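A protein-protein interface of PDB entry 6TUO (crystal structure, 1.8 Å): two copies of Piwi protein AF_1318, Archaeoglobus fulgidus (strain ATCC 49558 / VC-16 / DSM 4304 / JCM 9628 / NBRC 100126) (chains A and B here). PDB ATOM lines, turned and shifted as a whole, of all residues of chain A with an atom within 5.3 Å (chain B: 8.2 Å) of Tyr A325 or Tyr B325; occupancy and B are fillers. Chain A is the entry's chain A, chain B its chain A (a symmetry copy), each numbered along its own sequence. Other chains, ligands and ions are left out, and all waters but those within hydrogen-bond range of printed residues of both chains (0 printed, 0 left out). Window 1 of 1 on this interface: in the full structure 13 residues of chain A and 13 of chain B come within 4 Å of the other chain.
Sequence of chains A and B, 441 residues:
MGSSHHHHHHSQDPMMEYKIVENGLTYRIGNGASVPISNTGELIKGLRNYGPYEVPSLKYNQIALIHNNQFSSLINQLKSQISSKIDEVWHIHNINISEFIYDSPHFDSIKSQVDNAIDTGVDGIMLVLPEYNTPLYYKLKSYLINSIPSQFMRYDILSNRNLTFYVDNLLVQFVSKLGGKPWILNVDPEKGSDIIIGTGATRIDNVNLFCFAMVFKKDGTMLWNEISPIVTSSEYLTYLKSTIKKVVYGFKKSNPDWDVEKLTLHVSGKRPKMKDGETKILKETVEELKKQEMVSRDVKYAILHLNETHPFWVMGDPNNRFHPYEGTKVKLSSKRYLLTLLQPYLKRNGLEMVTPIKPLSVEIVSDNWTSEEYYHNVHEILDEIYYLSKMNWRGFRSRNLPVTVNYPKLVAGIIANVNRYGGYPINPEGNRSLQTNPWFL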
ATOM      1  N   VAL A 314     -28.851  27.993  -2.405  1.00  0.00           N
ATOM      2  CA  VAL A 314     -29.095  28.826  -1.234  1.00  0.00           C
ATOM      3  C   VAL A 314     -29.171  30.279  -1.691  1.00  0.00           C
ATOM      4  O   VAL A 314     -28.224  30.801  -2.287  1.00  0.00           O
ATOM      5  CB  VAL A 314     -28.004  28.632  -0.174  1.00  0.00           C
ATOM      6  CG1 VAL A 314     -28.308  29.468   1.053  1.00  0.00           C
ATOM      7  CG2 VAL A 314     -27.880  27.162   0.191  1.00  0.00           C
ATOM      8  N   HIS A 323     -18.895  29.822   1.742  1.00  0.00           N
ATOM      9  CA  HIS A 323     -18.340  28.865   2.697  1.00  0.00           C
ATOM     10  C   HIS A 323     -19.204  28.392   3.897  1.00  0.00           C
ATOM     11  O   HIS A 323     -18.741  27.538   4.653  1.00  0.00           O
ATOM     12  CB  HIS A 323     -17.026  29.430   3.252  1.00  0.00           C
ATOM     13  CG  HIS A 323     -17.200  30.318   4.445  1.00  0.00           C
ATOM     14  ND1 HIS A 323     -17.500  31.659   4.338  1.00  0.00           N
ATOM     15  CD2 HIS A 323     -17.102  30.060   5.771  1.00  0.00           C
ATOM     16  CE1 HIS A 323     -17.586  32.187   5.546  1.00  0.00           C
ATOM     17  NE2 HIS A 323     -17.350  31.238   6.433  1.00  0.00           N
ATOM     18  N   PRO A 324     -20.429  28.908   4.101  1.00  0.00           N
ATOM     19  CA  PRO A 324     -21.265  28.337   5.173  1.00  0.00           C
ATOM     20  C   PRO A 324     -21.674  26.894   4.935  1.00  0.00           C
ATOM     21  O   PRO A 324     -22.184  26.257   5.867  1.00  0.00           O
ATOM     22  CB  PRO A 324     -22.493  29.260   5.199  1.00  0.00           C
ATOM     23  CG  PRO A 324     -22.031  30.518   4.606  1.00  0.00           C
ATOM     24  CD  PRO A 324     -21.072  30.111   3.539  1.00  0.00           C
ATOM     25  N   TYR A 325     -21.471  26.356   3.735  1.00  0.00           N
ATOM     26  CA  TYR A 325     -21.858  24.986   3.430  1.00  0.00           C
ATOM     27  C   TYR A 325     -20.703  24.146   2.910  1.00  0.00           C
ATOM     28  O   TYR A 325     -20.915  22.982   2.544  1.00  0.00           O
ATOM     29  CB  TYR A 325     -23.019  24.983   2.430  1.00  0.00           C
ATOM     30  CG  TYR A 325     -24.174  25.808   2.939  1.00  0.00           C
ATOM     31  CD1 TYR A 325     -24.254  27.169   2.676  1.00  0.00           C
ATOM     32  CD2 TYR A 325     -25.157  25.234   3.730  1.00  0.00           C
ATOM     33  CE1 TYR A 325     -25.296  27.930   3.164  1.00  0.00           C
ATOM     34  CE2 TYR A 325     -26.203  25.987   4.220  1.00  0.00           C
ATOM     35  CZ  TYR A 325     -26.268  27.334   3.935  1.00  0.00           C
ATOM     36  OH  TYR A 325     -27.309  28.087   4.423  1.00  0.00           O
ATOM     37  N   GLU A 326     -19.491  24.694   2.880  1.00  0.00           N
ATOM     38  CA  GLU A 326     -18.303  23.911   2.571  1.00  0.00           C
ATOM     39  C   GLU A 326     -18.090  22.859   3.651  1.00  0.00           C
ATOM     40  O   GLU A 326     -17.542  23.158   4.718  1.00  0.00           O
ATOM     41  CB  GLU A 326     -17.075  24.817   2.454  1.00  0.00           C
ATOM     42  CG  GLU A 326     -16.570  25.004   1.034  1.00  0.00           C
ATOM     43  CD  GLU A 326     -16.197  23.693   0.369  1.00  0.00           C
ATOM     44  OE1 GLU A 326     -16.891  23.298  -0.589  1.00  0.00           O
ATOM     45  OE2 GLU A 326     -15.212  23.058   0.800  1.00  0.00           O
ATOM     46  N   GLY A 327     -18.535  21.635   3.395  1.00  0.00           N
ATOM     47  CA  GLY A 327     -18.362  20.549   4.333  1.00  0.00           C
ATOM     48  C   GLY A 327     -19.514  20.307   5.281  1.00  0.00           C
ATOM     49  O   GLY A 327     -19.332  19.587   6.268  1.00  0.00           O
ATOM     50  N   THR A 328     -20.691  20.866   5.010  1.00  0.00           N
ATOM     51  CA  THR A 328     -21.823  20.724   5.914  1.00  0.00           C
ATOM     52  C   THR A 328     -22.461  19.349   5.766  1.00  0.00           C
ATOM     53  O   THR A 328     -22.658  18.854   4.654  1.00  0.00           O
ATOM     54  CB  THR A 328     -22.854  21.822   5.646  1.00  0.00           C
ATOM     55  OG1 THR A 328     -22.319  23.076   6.085  1.00  0.00           O
ATOM     56  CG2 THR A 328     -24.173  21.542   6.384  1.00  0.00           C
ATOM     57  N   THR A 340     -23.556  18.653   1.551  1.00  0.00           N
ATOM     58  CA  THR A 340     -23.876  19.796   0.698  1.00  0.00           C
ATOM     59  C   THR A 340     -22.594  20.263   0.013  1.00  0.00           C
ATOM     60  O   THR A 340     -22.005  21.290   0.344  1.00  0.00           O
ATOM     61  CB  THR A 340     -24.527  20.913   1.505  1.00  0.00           C
ATOM     62  OG1 THR A 340     -23.585  21.429   2.451  1.00  0.00           O
ATOM     63  CG2 THR A 340     -25.750  20.390   2.252  1.00  0.00           C
ATOM     64  N   LEU A 341     -22.167  19.483  -0.973  1.00  0.00           N
ATOM     65  CA  LEU A 341     -20.998  19.847  -1.759  1.00  0.00           C
ATOM     66  C   LEU A 341     -21.292  21.074  -2.613  1.00  0.00           C
ATOM     67  O   LEU A 341     -22.368  21.199  -3.208  1.00  0.00           O
ATOM     68  CB  LEU A 341     -20.575  18.672  -2.643  1.00  0.00           C
ATOM     69  CG  LEU A 341     -20.314  17.382  -1.871  1.00  0.00           C
ATOM     70  CD1 LEU A 341     -19.859  16.256  -2.808  1.00  0.00           C
ATOM     71  CD2 LEU A 341     -19.279  17.637  -0.775  1.00  0.00           C
ATOM     72  N   LEU A 342     -20.329  21.987  -2.670  1.00  0.00           N
ATOM     73  CA  LEU A 342     -20.491  23.199  -3.460  1.00  0.00           C
ATOM     74  C   LEU A 342     -20.286  22.896  -4.936  1.00  0.00           C
ATOM     75  O   LEU A 342     -19.371  22.156  -5.312  1.00  0.00           O
ATOM     76  CB  LEU A 342     -19.501  24.276  -3.016  1.00  0.00           C
ATOM     77  CG  LEU A 342     -20.043  25.352  -2.074  1.00  0.00           C
ATOM     78  CD1 LEU A 342     -20.367  24.764  -0.709  1.00  0.00           C
ATOM     79  CD2 LEU A 342     -19.059  26.505  -1.950  1.00  0.00           C
ATOM     80  N   ILE A 357     -25.500  24.403  -4.833  1.00  0.00           N
ATOM     81  CA  ILE A 357     -25.132  23.203  -4.093  1.00  0.00           C
ATOM     82  C   ILE A 357     -25.291  22.000  -5.013  1.00  0.00           C
ATOM     83  O   ILE A 357     -26.272  21.904  -5.757  1.00  0.00           O
ATOM     84  CB  ILE A 357     -25.997  23.038  -2.826  1.00  0.00           C
ATOM     85  CG1 ILE A 357     -25.799  24.225  -1.878  1.00  0.00           C
ATOM     86  CG2 ILE A 357     -25.692  21.725  -2.123  1.00  0.00           C
ATOM     87  CD1 ILE A 357     -24.368  24.436  -1.459  1.00  0.00           C
ATOM     88  N   PHE B 312     -35.166  17.475   9.572  1.00  0.00           N
ATOM     89  CA  PHE B 312     -33.806  16.975   9.442  1.00  0.00           C
ATOM     90  C   PHE B 312     -32.894  17.763  10.373  1.00  0.00           C
ATOM     91  O   PHE B 312     -33.299  18.756  10.986  1.00  0.00           O
ATOM     92  CB  PHE B 312     -33.325  17.013   7.983  1.00  0.00           C
ATOM     93  CG  PHE B 312     -33.278  18.388   7.369  1.00  0.00           C
ATOM     94  CD1 PHE B 312     -32.249  19.269   7.658  1.00  0.00           C
ATOM     95  CD2 PHE B 312     -34.242  18.777   6.457  1.00  0.00           C
ATOM     96  CE1 PHE B 312     -32.201  20.521   7.070  1.00  0.00           C
ATOM     97  CE2 PHE B 312     -34.195  20.024   5.866  1.00  0.00           C
ATOM     98  CZ  PHE B 312     -33.180  20.895   6.175  1.00  0.00           C
ATOM     99  N   TRP B 313     -31.647  17.305  10.473  1.00  0.00           N
ATOM    100  CA  TRP B 313     -30.712  17.816  11.469  1.00  0.00           C
ATOM    101  C   TRP B 313     -29.384  18.167  10.821  1.00  0.00           C
ATOM    102  O   TRP B 313     -28.793  17.339  10.121  1.00  0.00           O
ATOM    103  CB  TRP B 313     -30.494  16.782  12.581  1.00  0.00           C
ATOM    104  CG  TRP B 313     -31.751  16.416  13.292  1.00  0.00           C
ATOM    105  CD1 TRP B 313     -32.233  16.971  14.441  1.00  0.00           C
ATOM    106  CD2 TRP B 313     -32.714  15.434  12.885  1.00  0.00           C
ATOM    107  NE1 TRP B 313     -33.426  16.386  14.783  1.00  0.00           N
ATOM    108  CE2 TRP B 313     -33.743  15.438  13.845  1.00  0.00           C
ATOM    109  CE3 TRP B 313     -32.800  14.545  11.808  1.00  0.00           C
ATOM    110  CZ2 TRP B 313     -34.845  14.594  13.758  1.00  0.00           C
ATOM    111  CZ3 TRP B 313     -33.889  13.710  11.724  1.00  0.00           C
ATOM    112  CH2 TRP B 313     -34.901  13.738  12.694  1.00  0.00           C
ATOM    113  N   VAL B 314     -28.909  19.381  11.072  1.00  0.00           N
ATOM    114  CA  VAL B 314     -27.558  19.774  10.689  1.00  0.00           C
ATOM    115  C   VAL B 314     -26.598  19.301  11.776  1.00  0.00           C
ATOM    116  O   VAL B 314     -26.741  19.671  12.945  1.00  0.00           O
ATOM    117  CB  VAL B 314     -27.457  21.290  10.478  1.00  0.00           C
ATOM    118  CG1 VAL B 314     -26.059  21.667  10.031  1.00  0.00           C
ATOM    119  CG2 VAL B 314     -28.491  21.752   9.466  1.00  0.00           C
ATOM    120  N   MET B 315     -25.617  18.485  11.392  1.00  0.00           N
ATOM    121  CA  MET B 315     -24.702  17.892  12.364  1.00  0.00           C
ATOM    122  C   MET B 315     -23.539  18.825  12.688  1.00  0.00           C
ATOM    123  O   MET B 315     -23.054  19.548  11.820  1.00  0.00           O
ATOM    124  CB  MET B 315     -24.176  16.552  11.845  1.00  0.00           C
ATOM    125  CG  MET B 315     -25.279  15.599  11.418  1.00  0.00           C
ATOM    126  SD  MET B 315     -24.664  14.099  10.625  1.00  0.00           S
ATOM    127  CE  MET B 315     -23.799  13.323  11.990  1.00  0.00           C
ATOM    128  N   HIS B 323     -27.947  29.655  14.705  1.00  0.00           N
ATOM    129  CA  HIS B 323     -28.375  30.753  13.841  1.00  0.00           C
ATOM    130  C   HIS B 323     -27.900  30.794  12.363  1.00  0.00           C
ATOM    131  O   HIS B 323     -28.323  31.693  11.636  1.00  0.00           O
ATOM    132  CB  HIS B 323     -27.982  32.080  14.503  1.00  0.00           C
ATOM    133  CG  HIS B 323     -26.594  32.538  14.174  1.00  0.00           C
ATOM    134  ND1 HIS B 323     -25.483  32.096  14.859  1.00  0.00           N
ATOM    135  CD2 HIS B 323     -26.139  33.409  13.242  1.00  0.00           C
ATOM    136  CE1 HIS B 323     -24.403  32.670  14.360  1.00  0.00           C
ATOM    137  NE2 HIS B 323     -24.773  33.471  13.377  1.00  0.00           N
ATOM    138  N   PRO B 324     -27.046  29.867  11.895  1.00  0.00           N
ATOM    139  CA  PRO B 324     -26.725  29.867  10.456  1.00  0.00           C
ATOM    140  C   PRO B 324     -27.908  29.545   9.559  1.00  0.00           C
ATOM    141  O   PRO B 324     -27.802  29.735   8.340  1.00  0.00           O
ATOM    142  CB  PRO B 324     -25.634  28.793  10.333  1.00  0.00           C
ATOM    143  CG  PRO B 324     -25.048  28.697  11.672  1.00  0.00           C
ATOM    144  CD  PRO B 324     -26.191  28.899  12.608  1.00  0.00           C
ATOM    145  N   TYR B 325     -29.024  29.072  10.109  1.00  0.00           N
ATOM    146  CA  TYR B 325     -30.188  28.722   9.309  1.00  0.00           C
ATOM    147  C   TYR B 325     -31.451  29.443   9.751  1.00  0.00           C
ATOM    148  O   TYR B 325     -32.527  29.178   9.199  1.00  0.00           O
ATOM    149  CB  TYR B 325     -30.399  27.204   9.330  1.00  0.00           C
ATOM    150  CG  TYR B 325     -29.154  26.478   8.885  1.00  0.00           C
ATOM    151  CD1 TYR B 325     -28.167  26.123   9.795  1.00  0.00           C
ATOM    152  CD2 TYR B 325     -28.942  26.197   7.544  1.00  0.00           C
ATOM    153  CE1 TYR B 325     -27.016  25.483   9.385  1.00  0.00           C
ATOM    154  CE2 TYR B 325     -27.796  25.555   7.126  1.00  0.00           C
ATOM    155  CZ  TYR B 325     -26.836  25.201   8.050  1.00  0.00           C
ATOM    156  OH  TYR B 325     -25.692  24.562   7.635  1.00  0.00           O
ATOM    157  N   GLU B 326     -31.349  30.352  10.718  1.00  0.00           N
ATOM    158  CA  GLU B 326     -32.464  31.215  11.079  1.00  0.00           C
ATOM    159  C   GLU B 326     -32.811  32.118   9.903  1.00  0.00           C
ATOM    160  O   GLU B 326     -32.161  33.147   9.690  1.00  0.00           O
ATOM    161  CB  GLU B 326     -32.121  32.050  12.315  1.00  0.00           C
ATOM    162  CG  GLU B 326     -32.845  31.620  13.579  1.00  0.00           C
ATOM    163  CD  GLU B 326     -34.354  31.672  13.435  1.00  0.00           C
ATOM    164  OE1 GLU B 326     -34.986  30.596  13.448  1.00  0.00           O
ATOM    165  OE2 GLU B 326     -34.909  32.783  13.310  1.00  0.00           O
ATOM    166  N   GLY B 327     -33.816  31.735   9.126  1.00  0.00           N
ATOM    167  CA  GLY B 327     -34.254  32.528   7.999  1.00  0.00           C
ATOM    168  C   GLY B 327     -33.646  32.166   6.663  1.00  0.00           C
ATOM    169  O   GLY B 327     -33.764  32.956   5.722  1.00  0.00           O
ATOM    170  N   THR B 328     -33.017  30.999   6.544  1.00  0.00           N
ATOM    171  CA  THR B 328     -32.356  30.618   5.304  1.00  0.00           C
ATOM    172  C   THR B 328     -33.376  30.156   4.270  1.00  0.00           C
ATOM    173  O   THR B 328     -34.303  29.405   4.581  1.00  0.00           O
ATOM    174  CB  THR B 328     -31.330  29.517   5.569  1.00  0.00           C
ATOM    175  OG1 THR B 328     -30.228  30.075   6.296  1.00  0.00           O
ATOM    176  CG2 THR B 328     -30.817  28.903   4.257  1.00  0.00           C
ATOM    177  N   LYS B 329     -33.202  30.623   3.038  1.00  0.00           N
ATOM    178  CA  LYS B 329     -34.106  30.319   1.937  1.00  0.00           C
ATOM    179  C   LYS B 329     -33.386  29.445   0.917  1.00  0.00           C
ATOM    180  O   LYS B 329     -32.291  29.794   0.461  1.00  0.00           O
ATOM    181  CB  LYS B 329     -34.601  31.610   1.277  1.00  0.00           C
ATOM    182  CG  LYS B 329     -35.282  32.563   2.249  1.00  0.00           C
ATOM    183  CD  LYS B 329     -35.456  33.962   1.670  1.00  0.00           C
ATOM    184  CE  LYS B 329     -34.220  34.821   1.918  1.00  0.00           C
ATOM    185  NZ  LYS B 329     -34.531  36.277   1.871  1.00  0.00           N
ATOM    186  N   VAL B 330     -34.002  28.321   0.552  1.00  0.00           N
ATOM    187  CA  VAL B 330     -33.437  27.387  -0.420  1.00  0.00           C
ATOM    188  C   VAL B 330     -34.312  27.387  -1.664  1.00  0.00           C
ATOM    189  O   VAL B 330     -35.531  27.210  -1.575  1.00  0.00           O
ATOM    190  CB  VAL B 330     -33.323  25.967   0.161  1.00  0.00           C
ATOM    191  CG1 VAL B 330     -32.836  24.981  -0.917  1.00  0.00           C
ATOM    192  CG2 VAL B 330     -32.408  25.946   1.367  1.00  0.00           C
ATOM    193  N   LEU B 339     -37.920  26.771   3.225  1.00  0.00           N
ATOM    194  CA  LEU B 339     -37.522  27.619   4.342  1.00  0.00           C
ATOM    195  C   LEU B 339     -37.080  26.723   5.490  1.00  0.00           C
ATOM    196  O   LEU B 339     -37.849  25.873   5.949  1.00  0.00           O
ATOM    197  CB  LEU B 339     -38.670  28.533   4.775  1.00  0.00           C
ATOM    198  CG  LEU B 339     -38.970  29.685   3.818  1.00  0.00           C
ATOM    199  CD1 LEU B 339     -40.286  30.358   4.186  1.00  0.00           C
ATOM    200  CD2 LEU B 339     -37.833  30.692   3.832  1.00  0.00           C
ATOM    201  N   THR B 340     -35.841  26.907   5.949  1.00  0.00           N
ATOM    202  CA  THR B 340     -35.272  26.038   6.979  1.00  0.00           C
ATOM    203  C   THR B 340     -35.596  26.634   8.346  1.00  0.00           C
ATOM    204  O   THR B 340     -34.750  27.198   9.038  1.00  0.00           O
ATOM    205  CB  THR B 340     -33.772  25.863   6.777  1.00  0.00           C
ATOM    206  OG1 THR B 340     -33.114  27.120   6.971  1.00  0.00           O
ATOM    207  CG2 THR B 340     -33.478  25.357   5.368  1.00  0.00           C
ATOM    208  N   LEU B 341     -36.856  26.490   8.739  1.00  0.00           N
ATOM    209  CA  LEU B 341     -37.286  26.946  10.052  1.00  0.00           C
ATOM    210  C   LEU B 341     -36.657  26.089  11.145  1.00  0.00           C
ATOM    211  O   LEU B 341     -36.576  24.862  11.030  1.00  0.00           O
ATOM    212  CB  LEU B 341     -38.812  26.898  10.150  1.00  0.00           C
ATOM    213  CG  LEU B 341     -39.525  27.687   9.055  1.00  0.00           C
ATOM    214  CD1 LEU B 341     -41.047  27.629   9.231  1.00  0.00           C
ATOM    215  CD2 LEU B 341     -39.026  29.132   9.053  1.00  0.00           C
ATOM    216  N   LEU B 342     -36.206  26.744  12.209  1.00  0.00           N
ATOM    217  CA  LEU B 342     -35.593  26.033  13.321  1.00  0.00           C
ATOM    218  C   LEU B 342     -36.661  25.378  14.181  1.00  0.00           C
ATOM    219  O   LEU B 342     -37.703  25.978  14.467  1.00  0.00           O
ATOM    220  CB  LEU B 342     -34.754  26.982  14.179  1.00  0.00           C
ATOM    221  CG  LEU B 342     -33.246  26.977  13.925  1.00  0.00           C
ATOM    222  CD1 LEU B 342     -32.925  27.562  12.559  1.00  0.00           C
ATOM    223  CD2 LEU B 342     -32.513  27.728  15.026  1.00  0.00           C
ATOM    224  N   THR B 355     -28.407  20.355  15.106  1.00  0.00           N
ATOM    225  CA  THR B 355     -29.382  21.434  15.135  1.00  0.00           C
ATOM    226  C   THR B 355     -30.630  20.976  14.401  1.00  0.00           C
ATOM    227  O   THR B 355     -30.544  20.662  13.201  1.00  0.00           O
ATOM    228  CB  THR B 355     -28.814  22.687  14.477  1.00  0.00           C
ATOM    229  OG1 THR B 355     -27.805  23.254  15.322  1.00  0.00           O
ATOM    230  CG2 THR B 355     -29.915  23.721  14.249  1.00  0.00           C
ATOM    231  N   PRO B 356     -31.788  20.887  15.056  1.00  0.00           N
ATOM    232  CA  PRO B 356     -32.986  20.402  14.361  1.00  0.00           C
ATOM    233  C   PRO B 356     -33.618  21.471  13.482  1.00  0.00           C
ATOM    234  O   PRO B 356     -33.777  22.628  13.881  1.00  0.00           O
ATOM    235  CB  PRO B 356     -33.926  19.996  15.505  1.00  0.00           C
ATOM    236  CG  PRO B 356     -33.477  20.791  16.670  1.00  0.00           C
ATOM    237  CD  PRO B 356     -32.000  21.031  16.507  1.00  0.00           C
ATOM    238  N   ILE B 357     -33.984  21.060  12.271  1.00  0.00           N
ATOM    239  CA  ILE B 357     -34.669  21.907  11.304  1.00  0.00           C
ATOM    240  C   ILE B 357     -36.080  21.371  11.106  1.00  0.00           C
ATOM    241  O   ILE B 357     -36.282  20.155  11.007  1.00  0.00           O
ATOM    242  CB  ILE B 357     -33.910  21.955   9.962  1.00  0.00           C
ATOM    243  CG1 ILE B 357     -32.508  22.542  10.154  1.00  0.00           C
ATOM    244  CG2 ILE B 357     -34.690  22.742   8.920  1.00  0.00           C
ATOM    245  CD1 ILE B 357     -32.504  23.922  10.757  1.00  0.00           C
ATOM    246  N   TYR B 386     -41.384  33.790   6.801  1.00  0.00           N
ATOM    247  CA  TYR B 386     -40.505  33.638   7.951  1.00  0.00           C
ATOM    248  C   TYR B 386     -40.971  34.520   9.104  1.00  0.00           C
ATOM    249  O   TYR B 386     -41.050  34.065  10.250  1.00  0.00           O
ATOM    250  CB  TYR B 386     -39.059  33.966   7.562  1.00  0.00           C
ATOM    251  CG  TYR B 386     -38.149  34.108   8.757  1.00  0.00           C
ATOM    252  CD1 TYR B 386     -37.744  32.994   9.480  1.00  0.00           C
ATOM    253  CD2 TYR B 386     -37.711  35.361   9.181  1.00  0.00           C
ATOM    254  CE1 TYR B 386     -36.914  33.121  10.585  1.00  0.00           C
ATOM    255  CE2 TYR B 386     -36.885  35.495  10.282  1.00  0.00           C
ATOM    256  CZ  TYR B 386     -36.490  34.373  10.978  1.00  0.00           C
ATOM    257  OH  TYR B 386     -35.671  34.512  12.075  1.00  0.00           O
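Tyr A325 touches its own counterpart, Tyr B325. Tyr A325 touches Thr B328, and with the chains exchanged Thr A328 touches Tyr B325.
The side-chain hydroxyl (OG1) of Thr B328 is in hydrogen-bond range of the backbone carbonyl oxygen (O) of Pro B324. The backbone carbonyl oxygen (O) of Tyr B325 sits at hydrogen-bond distance from the side-chain hydroxyl (OG1) of Thr B340, at 3.1 Å. The backbone NH of Thr B340 sits at hydrogen-bond distance from the backbone carbonyl oxygen of Thr B328. The backbone carbonyl oxygen (O) of Tyr A325 lies within hydrogen-bond range of the side-chain hydroxyl (OG1) of Thr A340, 3.1 Å away. The backbone carbonyl oxygen (O) of Thr A328 sits at hydrogen-bond distance from the backbone NH (N) of Thr A340, 3.2 Å away. O of Pro A324 lies within hydrogen-bond range of OG1 of Thr A328, 3.2 Å away.
Val A314 touches Lys B329. Tyr B325 touches Tyr A325 (CE2 to CE2, 3.3 Å). OH of Tyr A325 touches CG2 of Thr B328, at 3.6 Å. CG2 of Thr A328 touches OH of Tyr B325, at 3.6 Å.
Hydrophobic or aromatic side chains of chain B within 4 Å of the printed part of chain A: Tyr B325. Of the 11 printed residues of chain A, 3 touch a printed residue of chain B. Among the printed residues, no Asp or Glu carboxylate lies within 4 Å of a Lys or Arg side-chain nitrogen of the other chain.
Of the printed residues of chain B, Val A314 touches Lys B329. Printed residues of chain B within 4 Å of Tyr A325: Tyr B325 and Thr B328. Of the printed residues of chain A, Tyr B325 touches Tyr A325 (3.3 Å) and Thr A328 (3.6 Å). Printed residues of chain A within 4 Å of Lys B329: Val A314. The nearest residue of chain B that does not touch Tyr A325 is Pro B324 (4.3 Å).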
